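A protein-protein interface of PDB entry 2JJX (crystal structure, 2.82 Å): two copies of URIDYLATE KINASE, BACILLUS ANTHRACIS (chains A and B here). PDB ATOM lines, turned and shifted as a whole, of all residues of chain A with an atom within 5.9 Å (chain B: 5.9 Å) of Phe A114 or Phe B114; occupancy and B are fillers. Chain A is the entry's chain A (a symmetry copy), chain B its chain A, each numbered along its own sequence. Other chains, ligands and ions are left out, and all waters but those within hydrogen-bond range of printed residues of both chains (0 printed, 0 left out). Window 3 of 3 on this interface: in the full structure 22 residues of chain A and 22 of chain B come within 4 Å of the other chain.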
ATOM      1  N   LEU A  85      -9.540  15.589 -31.522  1.00  0.00           N
ATOM      2  CA  LEU A  85     -10.951  15.596 -31.901  1.00  0.00           C
ATOM      3  C   LEU A  85     -11.030  15.011 -33.309  1.00  0.00           C
ATOM      4  O   LEU A  85     -12.026  14.372 -33.665  1.00  0.00           O
ATOM      5  CB  LEU A  85     -11.514  17.022 -31.887  1.00  0.00           C
ATOM      6  CG  LEU A  85     -12.391  17.454 -30.714  1.00  0.00           C
ATOM      7  CD1 LEU A  85     -12.166  16.530 -29.531  1.00  0.00           C
ATOM      8  CD2 LEU A  85     -12.063  18.890 -30.332  1.00  0.00           C
ATOM      9  N   ILE A  88     -11.386  11.222 -33.380  1.00  0.00           N
ATOM     10  CA  ILE A  88     -12.738  10.776 -33.005  1.00  0.00           C
ATOM     11  C   ILE A  88     -13.691  10.860 -34.190  1.00  0.00           C
ATOM     12  O   ILE A  88     -14.550   9.987 -34.403  1.00  0.00           O
ATOM     13  CB  ILE A  88     -13.263  11.505 -31.781  1.00  0.00           C
ATOM     14  CG1 ILE A  88     -12.424  11.130 -30.563  1.00  0.00           C
ATOM     15  CG2 ILE A  88     -14.685  11.104 -31.466  1.00  0.00           C
ATOM     16  CD1 ILE A  88     -12.215  12.241 -29.622  1.00  0.00           C
ATOM     17  N   THR A 110     -13.992   6.171 -26.783  1.00  0.00           N
ATOM     18  CA  THR A 110     -13.189   7.390 -26.656  1.00  0.00           C
ATOM     19  C   THR A 110     -12.460   7.514 -25.318  1.00  0.00           C
ATOM     20  O   THR A 110     -12.889   7.001 -24.291  1.00  0.00           O
ATOM     21  CB  THR A 110     -14.018   8.667 -26.928  1.00  0.00           C
ATOM     22  OG1 THR A 110     -15.284   8.573 -26.260  1.00  0.00           O
ATOM     23  CG2 THR A 110     -14.252   8.831 -28.405  1.00  0.00           C
ATOM     24  N   ILE A 112     -11.941  10.411 -24.153  1.00  0.00           N
ATOM     25  CA  ILE A 112     -12.614  11.599 -23.666  1.00  0.00           C
ATOM     26  C   ILE A 112     -14.096  11.286 -23.811  1.00  0.00           C
ATOM     27  O   ILE A 112     -14.639  11.380 -24.912  1.00  0.00           O
ATOM     28  CB  ILE A 112     -12.242  12.809 -24.515  1.00  0.00           C
ATOM     29  CG1 ILE A 112     -10.733  13.045 -24.443  1.00  0.00           C
ATOM     30  CG2 ILE A 112     -12.996  14.003 -24.044  1.00  0.00           C
ATOM     31  CD1 ILE A 112     -10.222  13.908 -25.574  1.00  0.00           C
ATOM     32  N   PRO A 113     -14.697  10.686 -22.771  1.00  0.00           N
ATOM     33  CA  PRO A 113     -16.088  10.240 -22.878  1.00  0.00           C
ATOM     34  C   PRO A 113     -17.011  11.318 -23.412  1.00  0.00           C
ATOM     35  O   PRO A 113     -17.153  12.412 -22.839  1.00  0.00           O
ATOM     36  CB  PRO A 113     -16.446   9.821 -21.459  1.00  0.00           C
ATOM     37  CG  PRO A 113     -15.519  10.606 -20.603  1.00  0.00           C
ATOM     38  CD  PRO A 113     -14.289  10.925 -21.376  1.00  0.00           C
ATOM     39  N   PHE A 114     -17.525  11.042 -24.606  1.00  0.00           N
ATOM     40  CA  PHE A 114     -18.378  11.991 -25.317  1.00  0.00           C
ATOM     41  C   PHE A 114     -19.804  11.515 -25.115  1.00  0.00           C
ATOM     42  O   PHE A 114     -20.727  12.299 -24.990  1.00  0.00           O
ATOM     43  CB  PHE A 114     -18.001  12.091 -26.809  1.00  0.00           C
ATOM     44  CG  PHE A 114     -16.630  12.678 -27.022  1.00  0.00           C
ATOM     45  CD1 PHE A 114     -16.201  13.727 -26.214  1.00  0.00           C
ATOM     46  CD2 PHE A 114     -15.722  12.115 -27.898  1.00  0.00           C
ATOM     47  CE1 PHE A 114     -14.930  14.224 -26.301  1.00  0.00           C
ATOM     48  CE2 PHE A 114     -14.461  12.641 -28.014  1.00  0.00           C
ATOM     49  CZ  PHE A 114     -14.027  13.626 -27.143  1.00  0.00           C
ATOM     50  N   ASN A 115     -19.961  10.216 -24.905  1.00  0.00           N
ATOM     51  CA  ASN A 115     -21.274   9.618 -24.653  1.00  0.00           C
ATOM     52  C   ASN A 115     -22.293  10.065 -25.691  1.00  0.00           C
ATOM     53  O   ASN A 115     -22.261  11.193 -26.190  1.00  0.00           O
ATOM     54  CB  ASN A 115     -21.759   9.914 -23.231  1.00  0.00           C
ATOM     55  CG  ASN A 115     -21.316   8.860 -22.237  1.00  0.00           C
ATOM     56  OD1 ASN A 115     -21.936   7.805 -22.121  1.00  0.00           O
ATOM     57  ND2 ASN A 115     -20.250   9.147 -21.496  1.00  0.00           N
ATOM     58  N   ALA A 116     -23.197   9.159 -26.031  1.00  0.00           N
ATOM     59  CA  ALA A 116     -24.211   9.463 -27.024  1.00  0.00           C
ATOM     60  C   ALA A 116     -23.579   9.992 -28.312  1.00  0.00           C
ATOM     61  O   ALA A 116     -24.225  10.656 -29.120  1.00  0.00           O
ATOM     62  CB  ALA A 116     -25.238  10.424 -26.459  1.00  0.00           C
ATOM     63  N   VAL A 117     -22.295   9.685 -28.472  1.00  0.00           N
ATOM     64  CA  VAL A 117     -21.517   9.994 -29.670  1.00  0.00           C
ATOM     65  C   VAL A 117     -20.616   8.774 -29.844  1.00  0.00           C
ATOM     66  O   VAL A 117     -20.480   8.245 -30.946  1.00  0.00           O
ATOM     67  CB  VAL A 117     -20.694  11.258 -29.512  1.00  0.00           C
ATOM     68  CG1 VAL A 117     -19.218  10.916 -29.359  1.00  0.00           C
ATOM     69  CG2 VAL A 117     -20.928  12.228 -30.658  1.00  0.00           C
ATOM     70  N   ALA A 118     -20.092   8.282 -28.720  1.00  0.00           N
ATOM     71  CA  ALA A 118     -19.310   7.041 -28.650  1.00  0.00           C
ATOM     72  C   ALA A 118     -19.309   6.555 -27.196  1.00  0.00           C
ATOM     73  O   ALA A 118     -19.724   7.280 -26.295  1.00  0.00           O
ATOM     74  CB  ALA A 118     -17.893   7.257 -29.138  1.00  0.00           C
ATOM     75  N   GLU A 119     -18.854   5.332 -26.954  1.00  0.00           N
ATOM     76  CA  GLU A 119     -18.792   4.855 -25.583  1.00  0.00           C
ATOM     77  C   GLU A 119     -17.552   5.340 -24.866  1.00  0.00           C
ATOM     78  O   GLU A 119     -16.447   5.319 -25.414  1.00  0.00           O
ATOM     79  CB  GLU A 119     -18.871   3.330 -25.453  1.00  0.00           C
ATOM     80  CG  GLU A 119     -19.016   2.524 -26.722  1.00  0.00           C
ATOM     81  CD  GLU A 119     -19.398   1.070 -26.451  1.00  0.00           C
ATOM     82  OE1 GLU A 119     -19.027   0.506 -25.396  1.00  0.00           O
ATOM     83  OE2 GLU A 119     -20.091   0.484 -27.303  1.00  0.00           O
ATOM     84  N   PRO A 120     -17.713   5.715 -23.588  1.00  0.00           N
ATOM     85  CA  PRO A 120     -16.503   6.091 -22.857  1.00  0.00           C
ATOM     86  C   PRO A 120     -15.612   4.860 -22.812  1.00  0.00           C
ATOM     87  O   PRO A 120     -16.071   3.732 -22.699  1.00  0.00           O
ATOM     88  CB  PRO A 120     -17.026   6.430 -21.451  1.00  0.00           C
ATOM     89  CG  PRO A 120     -18.312   5.686 -21.353  1.00  0.00           C
ATOM     90  CD  PRO A 120     -18.897   5.728 -22.717  1.00  0.00           C
ATOM     91  N   LEU B  85     -18.714  17.505 -33.922  1.00  0.00           N
ATOM     92  CA  LEU B  85     -17.326  17.483 -33.467  1.00  0.00           C
ATOM     93  C   LEU B  85     -16.565  18.483 -34.335  1.00  0.00           C
ATOM     94  O   LEU B  85     -15.600  19.103 -33.875  1.00  0.00           O
ATOM     95  CB  LEU B  85     -16.722  16.082 -33.618  1.00  0.00           C
ATOM     96  CG  LEU B  85     -16.569  15.211 -32.374  1.00  0.00           C
ATOM     97  CD1 LEU B  85     -17.479  15.719 -31.271  1.00  0.00           C
ATOM     98  CD2 LEU B  85     -16.909  13.767 -32.716  1.00  0.00           C
ATOM     99  N   ILE B  88     -16.596  22.037 -32.973  1.00  0.00           N
ATOM    100  CA  ILE B  88     -15.703  22.204 -31.815  1.00  0.00           C
ATOM    101  C   ILE B  88     -14.262  22.416 -32.259  1.00  0.00           C
ATOM    102  O   ILE B  88     -13.511  23.223 -31.684  1.00  0.00           O
ATOM    103  CB  ILE B  88     -15.844  21.070 -30.814  1.00  0.00           C
ATOM    104  CG1 ILE B  88     -17.236  21.110 -30.189  1.00  0.00           C
ATOM    105  CG2 ILE B  88     -14.857  21.207 -29.679  1.00  0.00           C
ATOM    106  CD1 ILE B  88     -17.806  19.780 -29.925  1.00  0.00           C
ATOM    107  N   THR B 110     -18.417  24.399 -24.792  1.00  0.00           N
ATOM    108  CA  THR B 110     -19.041  23.289 -25.517  1.00  0.00           C
ATOM    109  C   THR B 110     -20.356  22.810 -24.901  1.00  0.00           C
ATOM    110  O   THR B 110     -20.593  22.918 -23.703  1.00  0.00           O
ATOM    111  CB  THR B 110     -18.075  22.095 -25.701  1.00  0.00           C
ATOM    112  OG1 THR B 110     -17.377  21.844 -24.473  1.00  0.00           O
ATOM    113  CG2 THR B 110     -17.075  22.396 -26.782  1.00  0.00           C
ATOM    114  N   ILE B 112     -21.132  19.756 -25.206  1.00  0.00           N
ATOM    115  CA  ILE B 112     -20.711  18.415 -24.852  1.00  0.00           C
ATOM    116  C   ILE B 112     -19.419  18.613 -24.073  1.00  0.00           C
ATOM    117  O   ILE B 112     -18.366  18.828 -24.673  1.00  0.00           O
ATOM    118  CB  ILE B 112     -20.453  17.588 -26.106  1.00  0.00           C
ATOM    119  CG1 ILE B 112     -21.736  17.489 -26.931  1.00  0.00           C
ATOM    120  CG2 ILE B 112     -19.954  16.238 -25.722  1.00  0.00           C
ATOM    121  CD1 ILE B 112     -21.478  17.093 -28.367  1.00  0.00           C
ATOM    122  N   PRO B 113     -19.527  18.782 -22.745  1.00  0.00           N
ATOM    123  CA  PRO B 113     -18.345  19.101 -21.942  1.00  0.00           C
ATOM    124  C   PRO B 113     -17.180  18.170 -22.215  1.00  0.00           C
ATOM    125  O   PRO B 113     -17.260  16.941 -22.047  1.00  0.00           O
ATOM    126  CB  PRO B 113     -18.842  19.001 -20.507  1.00  0.00           C
ATOM    127  CG  PRO B 113     -20.001  18.075 -20.587  1.00  0.00           C
ATOM    128  CD  PRO B 113     -20.592  18.144 -21.951  1.00  0.00           C
ATOM    129  N   PHE B 114     -16.137  18.767 -22.784  1.00  0.00           N
ATOM    130  CA  PHE B 114     -14.949  18.022 -23.192  1.00  0.00           C
ATOM    131  C   PHE B 114     -13.905  18.266 -22.120  1.00  0.00           C
ATOM    132  O   PHE B 114     -13.121  17.398 -21.784  1.00  0.00           O
ATOM    133  CB  PHE B 114     -14.460  18.447 -24.592  1.00  0.00           C
ATOM    134  CG  PHE B 114     -15.442  18.097 -25.680  1.00  0.00           C
ATOM    135  CD1 PHE B 114     -16.131  16.889 -25.617  1.00  0.00           C
ATOM    136  CD2 PHE B 114     -15.791  18.999 -26.666  1.00  0.00           C
ATOM    137  CE1 PHE B 114     -17.104  16.574 -26.525  1.00  0.00           C
ATOM    138  CE2 PHE B 114     -16.738  18.664 -27.601  1.00  0.00           C
ATOM    139  CZ  PHE B 114     -17.472  17.497 -27.470  1.00  0.00           C
ATOM    140  N   ASN B 115     -14.011  19.405 -21.451  1.00  0.00           N
ATOM    141  CA  ASN B 115     -13.101  19.758 -20.360  1.00  0.00           C
ATOM    142  C   ASN B 115     -11.647  19.575 -20.772  1.00  0.00           C
ATOM    143  O   ASN B 115     -11.299  18.678 -21.544  1.00  0.00           O
ATOM    144  CB  ASN B 115     -13.424  18.972 -19.086  1.00  0.00           C
ATOM    145  CG  ASN B 115     -14.428  19.685 -18.204  1.00  0.00           C
ATOM    146  OD1 ASN B 115     -14.072  20.579 -17.441  1.00  0.00           O
ATOM    147  ND2 ASN B 115     -15.692  19.278 -18.288  1.00  0.00           N
ATOM    148  N   ALA B 116     -10.795  20.450 -20.261  1.00  0.00           N
ATOM    149  CA  ALA B 116      -9.384  20.387 -20.594  1.00  0.00           C
ATOM    150  C   ALA B 116      -9.175  20.368 -22.109  1.00  0.00           C
ATOM    151  O   ALA B 116      -8.137  19.943 -22.611  1.00  0.00           O
ATOM    152  CB  ALA B 116      -8.729  19.200 -19.916  1.00  0.00           C
ATOM    153  N   VAL B 117     -10.199  20.833 -22.820  1.00  0.00           N
ATOM    154  CA  VAL B 117     -10.183  21.007 -24.271  1.00  0.00           C
ATOM    155  C   VAL B 117     -10.966  22.299 -24.492  1.00  0.00           C
ATOM    156  O   VAL B 117     -10.543  23.167 -25.254  1.00  0.00           O
ATOM    157  CB  VAL B 117     -10.836  19.846 -24.996  1.00  0.00           C
ATOM    158  CG1 VAL B 117     -12.191  20.262 -25.554  1.00  0.00           C
ATOM    159  CG2 VAL B 117      -9.934  19.282 -26.081  1.00  0.00           C
ATOM    160  N   ALA B 118     -12.054  22.449 -23.734  1.00  0.00           N
ATOM    161  CA  ALA B 118     -12.868  23.670 -23.694  1.00  0.00           C
ATOM    162  C   ALA B 118     -13.692  23.655 -22.402  1.00  0.00           C
ATOM    163  O   ALA B 118     -13.754  22.641 -21.712  1.00  0.00           O
ATOM    164  CB  ALA B 118     -13.778  23.762 -24.902  1.00  0.00           C
ATOM    165  N   GLU B 119     -14.323  24.772 -22.060  1.00  0.00           N
ATOM    166  CA  GLU B 119     -15.153  24.782 -20.867  1.00  0.00           C
ATOM    167  C   GLU B 119     -16.530  24.214 -21.126  1.00  0.00           C
ATOM    168  O   GLU B 119     -17.168  24.519 -22.137  1.00  0.00           O
ATOM    169  CB  GLU B 119     -15.303  26.168 -20.229  1.00  0.00           C
ATOM    170  CG  GLU B 119     -14.583  27.323 -20.882  1.00  0.00           C
ATOM    171  CD  GLU B 119     -14.548  28.568 -19.995  1.00  0.00           C
ATOM    172  OE1 GLU B 119     -15.477  28.792 -19.186  1.00  0.00           O
ATOM    173  OE2 GLU B 119     -13.568  29.327 -20.101  1.00  0.00           O
ATOM    174  N   PRO B 120     -17.040  23.432 -20.163  1.00  0.00           N
ATOM    175  CA  PRO B 120     -18.410  22.959 -20.360  1.00  0.00           C
ATOM    176  C   PRO B 120     -19.302  24.188 -20.401  1.00  0.00           C
ATOM    177  O   PRO B 120     -19.086  25.169 -19.702  1.00  0.00           O
ATOM    178  CB  PRO B 120     -18.688  22.133 -19.092  1.00  0.00           C
ATOM    179  CG  PRO B 120     -17.732  22.677 -18.089  1.00  0.00           C
ATOM    180  CD  PRO B 120     -16.509  23.023 -18.855  1.00  0.00           C
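CG2 of Ile B88 touches CD2 of Leu A85, 3.7 Å away.
Ile A88 touches Leu B85.
CE1 of Phe A114 touches CD1 of Phe B114, at 3.0 Å.
Of the printed residues of chain B, Leu A85 touches Ile B88.
Of the printed residues of chain B, Ile A88 touches Leu B85.
Of the printed residues of chain B, Phe A114 touches Phe B114.
Glu A119 touches none of the printed residues of chain B.
Of the printed residues of chain A, Phe B114 touches Phe A114 (3.0 Å).
The nearest printed residue of chain B that does not touch Ile A88 is Phe B114 (7.2 Å).
Of the 12 printed residues of chain B, 3 touch a printed residue of chain A.
Printed residues of chain B that touch a printed residue of chain A: Leu B85, Ile B88 and Phe B114.
Hydrophobic or aromatic side chains of chain A that line the printed part of chain B: Leu A85, Ile A88 and Phe A114.
Leu A85 touches Ile B88, and with the chains exchanged Ile A88 touches Leu B85.
Phe B114 touches its own counterpart, Phe A114.
Positions printed for both chains: 85, 88, 110, 112, 113, 114, 115, 116, 117, 118, 119 and 120.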
